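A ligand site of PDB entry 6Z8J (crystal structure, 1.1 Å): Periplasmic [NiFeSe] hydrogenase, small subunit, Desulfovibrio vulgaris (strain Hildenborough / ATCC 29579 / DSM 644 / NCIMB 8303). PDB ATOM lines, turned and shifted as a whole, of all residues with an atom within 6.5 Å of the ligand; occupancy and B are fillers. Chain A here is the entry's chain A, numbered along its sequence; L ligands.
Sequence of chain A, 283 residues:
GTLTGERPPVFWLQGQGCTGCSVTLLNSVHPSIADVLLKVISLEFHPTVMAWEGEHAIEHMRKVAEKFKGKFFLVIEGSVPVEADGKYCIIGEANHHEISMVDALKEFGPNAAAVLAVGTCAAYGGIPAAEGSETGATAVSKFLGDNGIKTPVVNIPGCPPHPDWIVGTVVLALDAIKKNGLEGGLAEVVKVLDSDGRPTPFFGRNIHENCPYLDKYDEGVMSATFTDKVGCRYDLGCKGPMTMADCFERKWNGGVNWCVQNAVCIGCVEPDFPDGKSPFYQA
SG of Cys 238 sits close to N of Gly 240 (3.4 Å).
NH2 of Arg 233 is in hydrogen-bond range of OH of Tyr 213.
O of Arg 233 is in hydrogen-bond range of N of Cys 238 (3.2 Å).
The backbone NH (N) of Tyr 234 sits close to the side-chain sulfur (SG) of Cys 232.
SG of Cys 211 sits close to N of Tyr 213, 3.4 Å away.
O of Gly 231 lies within hydrogen-bond range of NH1 of Arg 233, 2.8 Å away.
The guanidinium group of Arg 233 sits at hydrogen-bond distance from the backbone carbonyl oxygen of Val 260 (2.9 Å).
SG of Cys 232 sits close to SD of Met 222, 3.6 Å away.
S1 of the ligand lies close to O of Tyr 213, at 3.7 Å.
Tyr 217 touches the ligand (CB to S1, 3.8 Å).
Tyr 234 touches the ligand (CB to S4, 3.7 Å).
Gly 240 touches the ligand.
Pro 241 touches the ligand.
CG1 of Val 260 touches S2 of the ligand (3.5 Å).
Within 4 Å of the ligand: His 208, Cys 211, Tyr 213, Leu 214, Tyr 217, Cys 232, Arg 233, Tyr 234, Cys 238, Gly 240, Pro 241 and Val 260.
The backbone NH (N) of Arg 233 lies close to a sulfur (S2) of the ligand.
A sulfur (S1) of the ligand sits close to the backbone NH (N) of Leu 214 (3.6 Å).
ND1 of His 208 is bound to FE2 of the ligand, at 2.1 Å.
FE4 of the ligand is bound by SG of Cys 211, at 2.3 Å.
The side-chain sulfur of Cys 238 is bound to an iron atom (FE1) of the ligand (2.3 Å).
The side-chain sulfur of Cys 232 is bound to an iron atom (FE3) of the ligand, at 2.3 Å.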
ATOM      1  N   ILE A 207      -2.823 -12.598 -22.746  1.00  0.00           N
ATOM      2  CA  ILE A 207      -1.915 -13.716 -23.002  1.00  0.00           C
ATOM      3  C   ILE A 207      -2.588 -15.032 -22.636  1.00  0.00           C
ATOM      4  O   ILE A 207      -2.664 -15.964 -23.449  1.00  0.00           O
ATOM      5  CB  ILE A 207      -0.596 -13.537 -22.231  1.00  0.00           C
ATOM      6  CG1 ILE A 207       0.198 -12.310 -22.715  1.00  0.00           C
ATOM      7  CG2 ILE A 207       0.241 -14.816 -22.304  1.00  0.00           C
ATOM      8  CD1 ILE A 207       1.223 -12.587 -23.819  1.00  0.00           C
ATOM      9  N   HIS A 208      -3.058 -15.132 -21.399  1.00  0.00           N
ATOM     10  CA  HIS A 208      -3.573 -16.387 -20.856  1.00  0.00           C
ATOM     11  C   HIS A 208      -4.759 -16.921 -21.655  1.00  0.00           C
ATOM     12  O   HIS A 208      -4.825 -18.106 -21.969  1.00  0.00           O
ATOM     13  CB  HIS A 208      -3.949 -16.109 -19.403  1.00  0.00           C
ATOM     14  CG  HIS A 208      -4.606 -17.233 -18.669  1.00  0.00           C
ATOM     15  ND1 HIS A 208      -3.933 -18.345 -18.213  1.00  0.00           N
ATOM     16  CD2 HIS A 208      -5.886 -17.376 -18.241  1.00  0.00           C
ATOM     17  CE1 HIS A 208      -4.768 -19.132 -17.570  1.00  0.00           C
ATOM     18  NE2 HIS A 208      -5.958 -18.569 -17.590  1.00  0.00           N
ATOM     19  N   GLU A 209      -5.697 -16.045 -22.000  1.00  0.00           N
ATOM     20  CA  GLU A 209      -6.863 -16.498 -22.771  1.00  0.00           C
ATOM     21  C   GLU A 209      -6.458 -17.102 -24.116  1.00  0.00           C
ATOM     22  O   GLU A 209      -7.233 -17.875 -24.693  1.00  0.00           O
ATOM     23  CB  GLU A 209      -7.793 -15.316 -23.007  1.00  0.00           C
ATOM     24  CG  GLU A 209      -8.475 -14.805 -21.743  1.00  0.00           C
ATOM     25  CD  GLU A 209      -9.194 -13.481 -21.948  1.00  0.00           C
ATOM     26  OE1 GLU A 209      -9.339 -12.728 -20.958  1.00  0.00           O
ATOM     27  OE2 GLU A 209      -9.585 -13.187 -23.102  1.00  0.00           O
ATOM     28  N   CYS A 211      -3.294 -18.614 -24.626  1.00  0.00           N
ATOM     29  CA  CYS A 211      -2.052 -19.324 -24.409  1.00  0.00           C
ATOM     30  C   CYS A 211      -2.173 -20.786 -24.850  1.00  0.00           C
ATOM     31  O   CYS A 211      -3.200 -21.417 -24.609  1.00  0.00           O
ATOM     32  CB  CYS A 211      -1.690 -19.288 -22.919  1.00  0.00           C
ATOM     33  SG  CYS A 211      -0.173 -20.174 -22.522  1.00  0.00           S
ATOM     34  N   PRO A 212      -1.134 -21.338 -25.481  1.00  0.00           N
ATOM     35  CA  PRO A 212      -1.182 -22.763 -25.860  1.00  0.00           C
ATOM     36  C   PRO A 212      -1.283 -23.736 -24.687  1.00  0.00           C
ATOM     37  O   PRO A 212      -1.676 -24.892 -24.915  1.00  0.00           O
ATOM     38  CB  PRO A 212       0.103 -22.956 -26.674  1.00  0.00           C
ATOM     39  CG  PRO A 212       1.005 -21.865 -26.238  1.00  0.00           C
ATOM     40  CD  PRO A 212       0.118 -20.697 -25.913  1.00  0.00           C
ATOM     41  N   TYR A 213      -0.968 -23.322 -23.473  1.00  0.00           N
ATOM     42  CA  TYR A 213      -1.045 -24.185 -22.292  1.00  0.00           C
ATOM     43  C   TYR A 213      -2.331 -24.009 -21.497  1.00  0.00           C
ATOM     44  O   TYR A 213      -2.458 -24.550 -20.394  1.00  0.00           O
ATOM     45  CB  TYR A 213       0.192 -23.972 -21.400  1.00  0.00           C
ATOM     46  CG  TYR A 213       1.439 -24.035 -22.214  1.00  0.00           C
ATOM     47  CD1 TYR A 213       1.841 -25.221 -22.813  1.00  0.00           C
ATOM     48  CD2 TYR A 213       2.201 -22.904 -22.428  1.00  0.00           C
ATOM     49  CE1 TYR A 213       2.962 -25.275 -23.602  1.00  0.00           C
ATOM     50  CE2 TYR A 213       3.334 -22.940 -23.207  1.00  0.00           C
ATOM     51  CZ  TYR A 213       3.708 -24.128 -23.796  1.00  0.00           C
ATOM     52  OH  TYR A 213       4.841 -24.124 -24.561  1.00  0.00           O
ATOM     53  N   LEU A 214      -3.295 -23.243 -22.037  1.00  0.00           N
ATOM     54  CA  LEU A 214      -4.524 -22.971 -21.305  1.00  0.00           C
ATOM     55  C   LEU A 214      -5.266 -24.251 -20.950  1.00  0.00           C
ATOM     56  O   LEU A 214      -5.857 -24.345 -19.867  1.00  0.00           O
ATOM     57  CB  LEU A 214      -5.409 -22.016 -22.106  1.00  0.00           C
ATOM     58  CG  LEU A 214      -6.700 -21.542 -21.408  1.00  0.00           C
ATOM     59  CD1 LEU A 214      -6.429 -20.799 -20.101  1.00  0.00           C
ATOM     60  CD2 LEU A 214      -7.504 -20.662 -22.342  1.00  0.00           C
ATOM     61  N   ASP A 215      -5.241 -25.247 -21.841  1.00  0.00           N
ATOM     62  CA  ASP A 215      -5.864 -26.536 -21.532  1.00  0.00           C
ATOM     63  C   ASP A 215      -5.253 -27.144 -20.273  1.00  0.00           C
ATOM     64  O   ASP A 215      -5.973 -27.668 -19.409  1.00  0.00           O
ATOM     65  CB  ASP A 215      -5.688 -27.491 -22.718  1.00  0.00           C
ATOM     66  CG  ASP A 215      -6.994 -28.147 -23.145  1.00  0.00           C
ATOM     67  OD1 ASP A 215      -7.759 -28.609 -22.261  1.00  0.00           O
ATOM     68  OD2 ASP A 215      -7.254 -28.204 -24.376  1.00  0.00           O
ATOM     69  N   LYS A 216      -3.924 -27.069 -20.138  1.00  0.00           N
ATOM     70  CA  LYS A 216      -3.268 -27.610 -18.943  1.00  0.00           C
ATOM     71  C   LYS A 216      -3.652 -26.816 -17.691  1.00  0.00           C
ATOM     72  O   LYS A 216      -3.868 -27.401 -16.627  1.00  0.00           O
ATOM     73  CB  LYS A 216      -1.755 -27.587 -19.136  1.00  0.00           C
ATOM     74  CG  LYS A 216      -1.289 -28.382 -20.347  1.00  0.00           C
ATOM     75  CD  LYS A 216      -1.620 -29.858 -20.210  1.00  0.00           C
ATOM     76  CE  LYS A 216      -0.912 -30.674 -21.276  1.00  0.00           C
ATOM     77  NZ  LYS A 216      -1.649 -31.896 -21.586  1.00  0.00           N
ATOM     78  N   TYR A 217      -3.726 -25.491 -17.800  1.00  0.00           N
ATOM     79  CA  TYR A 217      -4.201 -24.683 -16.684  1.00  0.00           C
ATOM     80  C   TYR A 217      -5.577 -25.155 -16.235  1.00  0.00           C
ATOM     81  O   TYR A 217      -5.814 -25.412 -15.057  1.00  0.00           O
ATOM     82  CB  TYR A 217      -4.251 -23.214 -17.093  1.00  0.00           C
ATOM     83  CG  TYR A 217      -4.814 -22.284 -16.060  1.00  0.00           C
ATOM     84  CD1 TYR A 217      -3.987 -21.641 -15.145  1.00  0.00           C
ATOM     85  CD2 TYR A 217      -6.166 -22.003 -16.015  1.00  0.00           C
ATOM     86  CE1 TYR A 217      -4.496 -20.770 -14.205  1.00  0.00           C
ATOM     87  CE2 TYR A 217      -6.688 -21.124 -15.076  1.00  0.00           C
ATOM     88  CZ  TYR A 217      -5.856 -20.513 -14.177  1.00  0.00           C
ATOM     89  OH  TYR A 217      -6.388 -19.639 -13.243  1.00  0.00           O
ATOM     90  N   ASP A 218      -6.498 -25.299 -17.194  1.00  0.00           N
ATOM     91  CA  ASP A 218      -7.861 -25.719 -16.871  1.00  0.00           C
ATOM     92  C   ASP A 218      -7.889 -27.109 -16.236  1.00  0.00           C
ATOM     93  O   ASP A 218      -8.769 -27.400 -15.422  1.00  0.00           O
ATOM     94  CB  ASP A 218      -8.715 -25.674 -18.133  1.00  0.00           C
ATOM     95  CG  ASP A 218      -9.112 -24.264 -18.539  1.00  0.00           C
ATOM     96  OD1 ASP A 218      -8.967 -23.323 -17.738  1.00  0.00           O
ATOM     97  OD2 ASP A 218      -9.586 -24.097 -19.687  1.00  0.00           O
ATOM     98  N   MET A 222       0.276 -28.694 -13.828  1.00  0.00           N
ATOM     99  CA  MET A 222       1.254 -27.639 -13.655  1.00  0.00           C
ATOM    100  C   MET A 222       2.674 -28.199 -13.659  1.00  0.00           C
ATOM    101  O   MET A 222       2.937 -29.261 -13.081  1.00  0.00           O
ATOM    102  CB  MET A 222       1.069 -26.931 -12.302  1.00  0.00           C
ATOM    103  CG  MET A 222      -0.262 -26.286 -12.123  1.00  0.00           C
ATOM    104  SD  MET A 222      -0.408 -24.904 -13.224  1.00  0.00           S
ATOM    105  CE  MET A 222      -2.161 -24.555 -13.111  1.00  0.00           C
ATOM    106  N   GLY A 231       3.439 -28.877 -18.708  1.00  0.00           N
ATOM    107  CA  GLY A 231       2.414 -28.282 -17.884  1.00  0.00           C
ATOM    108  C   GLY A 231       2.323 -26.775 -18.018  1.00  0.00           C
ATOM    109  O   GLY A 231       3.201 -26.109 -18.554  1.00  0.00           O
ATOM    110  N   CYS A 232       1.240 -26.256 -17.459  1.00  0.00           N
ATOM    111  CA  CYS A 232       1.084 -24.818 -17.311  1.00  0.00           C
ATOM    112  C   CYS A 232       2.126 -24.268 -16.337  1.00  0.00           C
ATOM    113  O   CYS A 232       2.590 -24.968 -15.423  1.00  0.00           O
ATOM    114  CB  CYS A 232      -0.345 -24.551 -16.822  1.00  0.00           C
ATOM    115  SG  CYS A 232      -0.656 -22.885 -16.250  1.00  0.00           S
ATOM    116  N   ARG A 233       2.509 -23.012 -16.559  1.00  0.00           N
ATOM    117  CA  ARG A 233       3.578 -22.332 -15.825  1.00  0.00           C
ATOM    118  C   ARG A 233       3.047 -21.487 -14.663  1.00  0.00           C
ATOM    119  O   ARG A 233       3.824 -20.768 -14.040  1.00  0.00           O
ATOM    120  CB  ARG A 233       4.386 -21.451 -16.772  1.00  0.00           C
ATOM    121  CG  ARG A 233       5.288 -22.168 -17.770  1.00  0.00           C
ATOM    122  CD  ARG A 233       4.609 -22.989 -18.831  1.00  0.00           C
ATOM    123  NE  ARG A 233       5.519 -23.138 -19.969  1.00  0.00           N
ATOM    124  CZ  ARG A 233       5.550 -24.156 -20.821  1.00  0.00           C
ATOM    125  NH1 ARG A 233       4.704 -25.173 -20.711  1.00  0.00           N
ATOM    126  NH2 ARG A 233       6.450 -24.152 -21.799  1.00  0.00           N
ATOM    127  N   TYR A 234       1.757 -21.576 -14.367  1.00  0.00           N
ATOM    128  CA  TYR A 234       1.158 -20.710 -13.343  1.00  0.00           C
ATOM    129  C   TYR A 234       1.853 -20.847 -12.000  1.00  0.00           C
ATOM    130  O   TYR A 234       2.156 -19.847 -11.331  1.00  0.00           O
ATOM    131  CB  TYR A 234      -0.331 -21.027 -13.213  1.00  0.00           C
ATOM    132  CG  TYR A 234      -1.035 -20.197 -12.185  1.00  0.00           C
ATOM    133  CD1 TYR A 234      -1.475 -18.922 -12.486  1.00  0.00           C
ATOM    134  CD2 TYR A 234      -1.265 -20.688 -10.900  1.00  0.00           C
ATOM    135  CE1 TYR A 234      -2.131 -18.158 -11.549  1.00  0.00           C
ATOM    136  CE2 TYR A 234      -1.926 -19.933  -9.962  1.00  0.00           C
ATOM    137  CZ  TYR A 234      -2.362 -18.668 -10.297  1.00  0.00           C
ATOM    138  OH  TYR A 234      -3.012 -17.918  -9.343  1.00  0.00           O
ATOM    139  N   ASP A 235       2.075 -22.078 -11.533  1.00  0.00           N
ATOM    140  CA  ASP A 235       2.664 -22.257 -10.215  1.00  0.00           C
ATOM    141  C   ASP A 235       4.116 -21.799 -10.167  1.00  0.00           C
ATOM    142  O   ASP A 235       4.628 -21.517  -9.081  1.00  0.00           O
ATOM    143  CB  ASP A 235       2.587 -23.730  -9.786  1.00  0.00           C
ATOM    144  CG  ASP A 235       1.196 -24.148  -9.317  1.00  0.00           C
ATOM    145  OD1 ASP A 235       0.283 -23.295  -9.264  1.00  0.00           O
ATOM    146  OD2 ASP A 235       1.015 -25.339  -8.979  1.00  0.00           O
ATOM    147  N   CYS A 238       3.888 -17.629 -13.642  1.00  0.00           N
ATOM    148  CA  CYS A 238       3.441 -16.983 -14.871  1.00  0.00           C
ATOM    149  C   CYS A 238       2.348 -15.954 -14.606  1.00  0.00           C
ATOM    150  O   CYS A 238       1.328 -16.255 -13.965  1.00  0.00           O
ATOM    151  CB  CYS A 238       2.907 -18.050 -15.822  1.00  0.00           C
ATOM    152  SG  CYS A 238       2.475 -17.360 -17.448  1.00  0.00           S
ATOM    153  N   LYS A 239       2.545 -14.751 -15.127  1.00  0.00           N
ATOM    154  CA  LYS A 239       1.576 -13.674 -14.983  1.00  0.00           C
ATOM    155  C   LYS A 239       0.729 -13.469 -16.232  1.00  0.00           C
ATOM    156  O   LYS A 239       0.061 -12.441 -16.349  1.00  0.00           O
ATOM    157  CB  LYS A 239       2.287 -12.369 -14.608  1.00  0.00           C
ATOM    158  CG  LYS A 239       3.119 -12.478 -13.312  1.00  0.00           C
ATOM    159  CD  LYS A 239       2.335 -13.065 -12.139  1.00  0.00           C
ATOM    160  CE  LYS A 239       3.096 -12.917 -10.822  1.00  0.00           C
ATOM    161  NZ  LYS A 239       4.431 -13.545 -10.903  1.00  0.00           N
ATOM    162  N   GLY A 240       0.741 -14.428 -17.165  1.00  0.00           N
ATOM    163  CA  GLY A 240      -0.132 -14.357 -18.309  1.00  0.00           C
ATOM    164  C   GLY A 240      -1.573 -14.008 -18.007  1.00  0.00           C
ATOM    165  O   GLY A 240      -2.187 -13.245 -18.777  1.00  0.00           O
ATOM    166  N   PRO A 241      -2.152 -14.528 -16.934  1.00  0.00           N
ATOM    167  CA  PRO A 241      -3.560 -14.232 -16.652  1.00  0.00           C
ATOM    168  C   PRO A 241      -3.867 -12.752 -16.528  1.00  0.00           C
ATOM    169  O   PRO A 241      -5.005 -12.344 -16.809  1.00  0.00           O
ATOM    170  CB  PRO A 241      -3.833 -15.001 -15.344  1.00  0.00           C
ATOM    171  CG  PRO A 241      -2.908 -16.169 -15.419  1.00  0.00           C
ATOM    172  CD  PRO A 241      -1.647 -15.601 -16.046  1.00  0.00           C
ATOM    173  N   TRP A 258       9.364 -17.450 -26.928  1.00  0.00           N
ATOM    174  CA  TRP A 258       8.700 -16.401 -26.158  1.00  0.00           C
ATOM    175  C   TRP A 258       8.761 -16.791 -24.694  1.00  0.00           C
ATOM    176  O   TRP A 258       9.101 -17.919 -24.337  1.00  0.00           O
ATOM    177  CB  TRP A 258       7.282 -16.120 -26.635  1.00  0.00           C
ATOM    178  CG  TRP A 258       6.272 -17.194 -26.415  1.00  0.00           C
ATOM    179  CD1 TRP A 258       6.296 -18.470 -26.903  1.00  0.00           C
ATOM    180  CD2 TRP A 258       5.034 -17.058 -25.701  1.00  0.00           C
ATOM    181  NE1 TRP A 258       5.158 -19.144 -26.535  1.00  0.00           N
ATOM    182  CE2 TRP A 258       4.363 -18.308 -25.793  1.00  0.00           C
ATOM    183  CE3 TRP A 258       4.414 -16.007 -25.005  1.00  0.00           C
ATOM    184  CZ2 TRP A 258       3.099 -18.522 -25.230  1.00  0.00           C
ATOM    185  CZ3 TRP A 258       3.168 -16.240 -24.410  1.00  0.00           C
ATOM    186  CH2 TRP A 258       2.524 -17.479 -24.534  1.00  0.00           C
ATOM    187  N   VAL A 260       6.702 -17.437 -22.195  1.00  0.00           N
ATOM    188  CA  VAL A 260       5.960 -18.525 -21.580  1.00  0.00           C
ATOM    189  C   VAL A 260       6.512 -19.872 -22.011  1.00  0.00           C
ATOM    190  O   VAL A 260       6.593 -20.806 -21.211  1.00  0.00           O
ATOM    191  CB  VAL A 260       4.455 -18.388 -21.855  1.00  0.00           C
ATOM    192  CG1 VAL A 260       3.660 -19.618 -21.385  1.00  0.00           C
ATOM    193  CG2 VAL A 260       3.917 -17.094 -21.213  1.00  0.00           C
ATOM    194  N   CYS A 265       5.867 -15.695 -18.120  1.00  0.00           N
ATOM    195  CA  CYS A 265       5.587 -14.273 -18.361  1.00  0.00           C
ATOM    196  C   CYS A 265       5.691 -13.518 -17.035  1.00  0.00           C
ATOM    197  O   CYS A 265       5.163 -13.970 -16.004  1.00  0.00           O
ATOM    198  CB  CYS A 265       4.180 -14.135 -18.942  1.00  0.00           C
ATOM    199  SG  CYS A 265       3.590 -12.417 -19.210  1.00  0.00           S
HETATM  200 FE1  LIG L   1       0.775 -18.781 -18.102  1.00  0.00          FE
HETATM  201 FE2  LIG L   1      -1.948 -18.979 -18.405  1.00  0.00          FE
HETATM  202 FE3  LIG L   1      -0.555 -21.202 -17.811  1.00  0.00          FE
HETATM  203 FE4  LIG L   1      -0.319 -20.032 -20.263  1.00  0.00          FE
HETATM  204  S1  LIG L   1      -2.172 -21.035 -19.404  1.00  0.00           S
HETATM  205  S2  LIG L   1       1.383 -20.849 -18.958  1.00  0.00           S
HETATM  206  S3  LIG L   1      -0.503 -17.787 -19.721  1.00  0.00           S
HETATM  207  S4  LIG L   1      -0.755 -19.308 -16.479  1.00  0.00           S
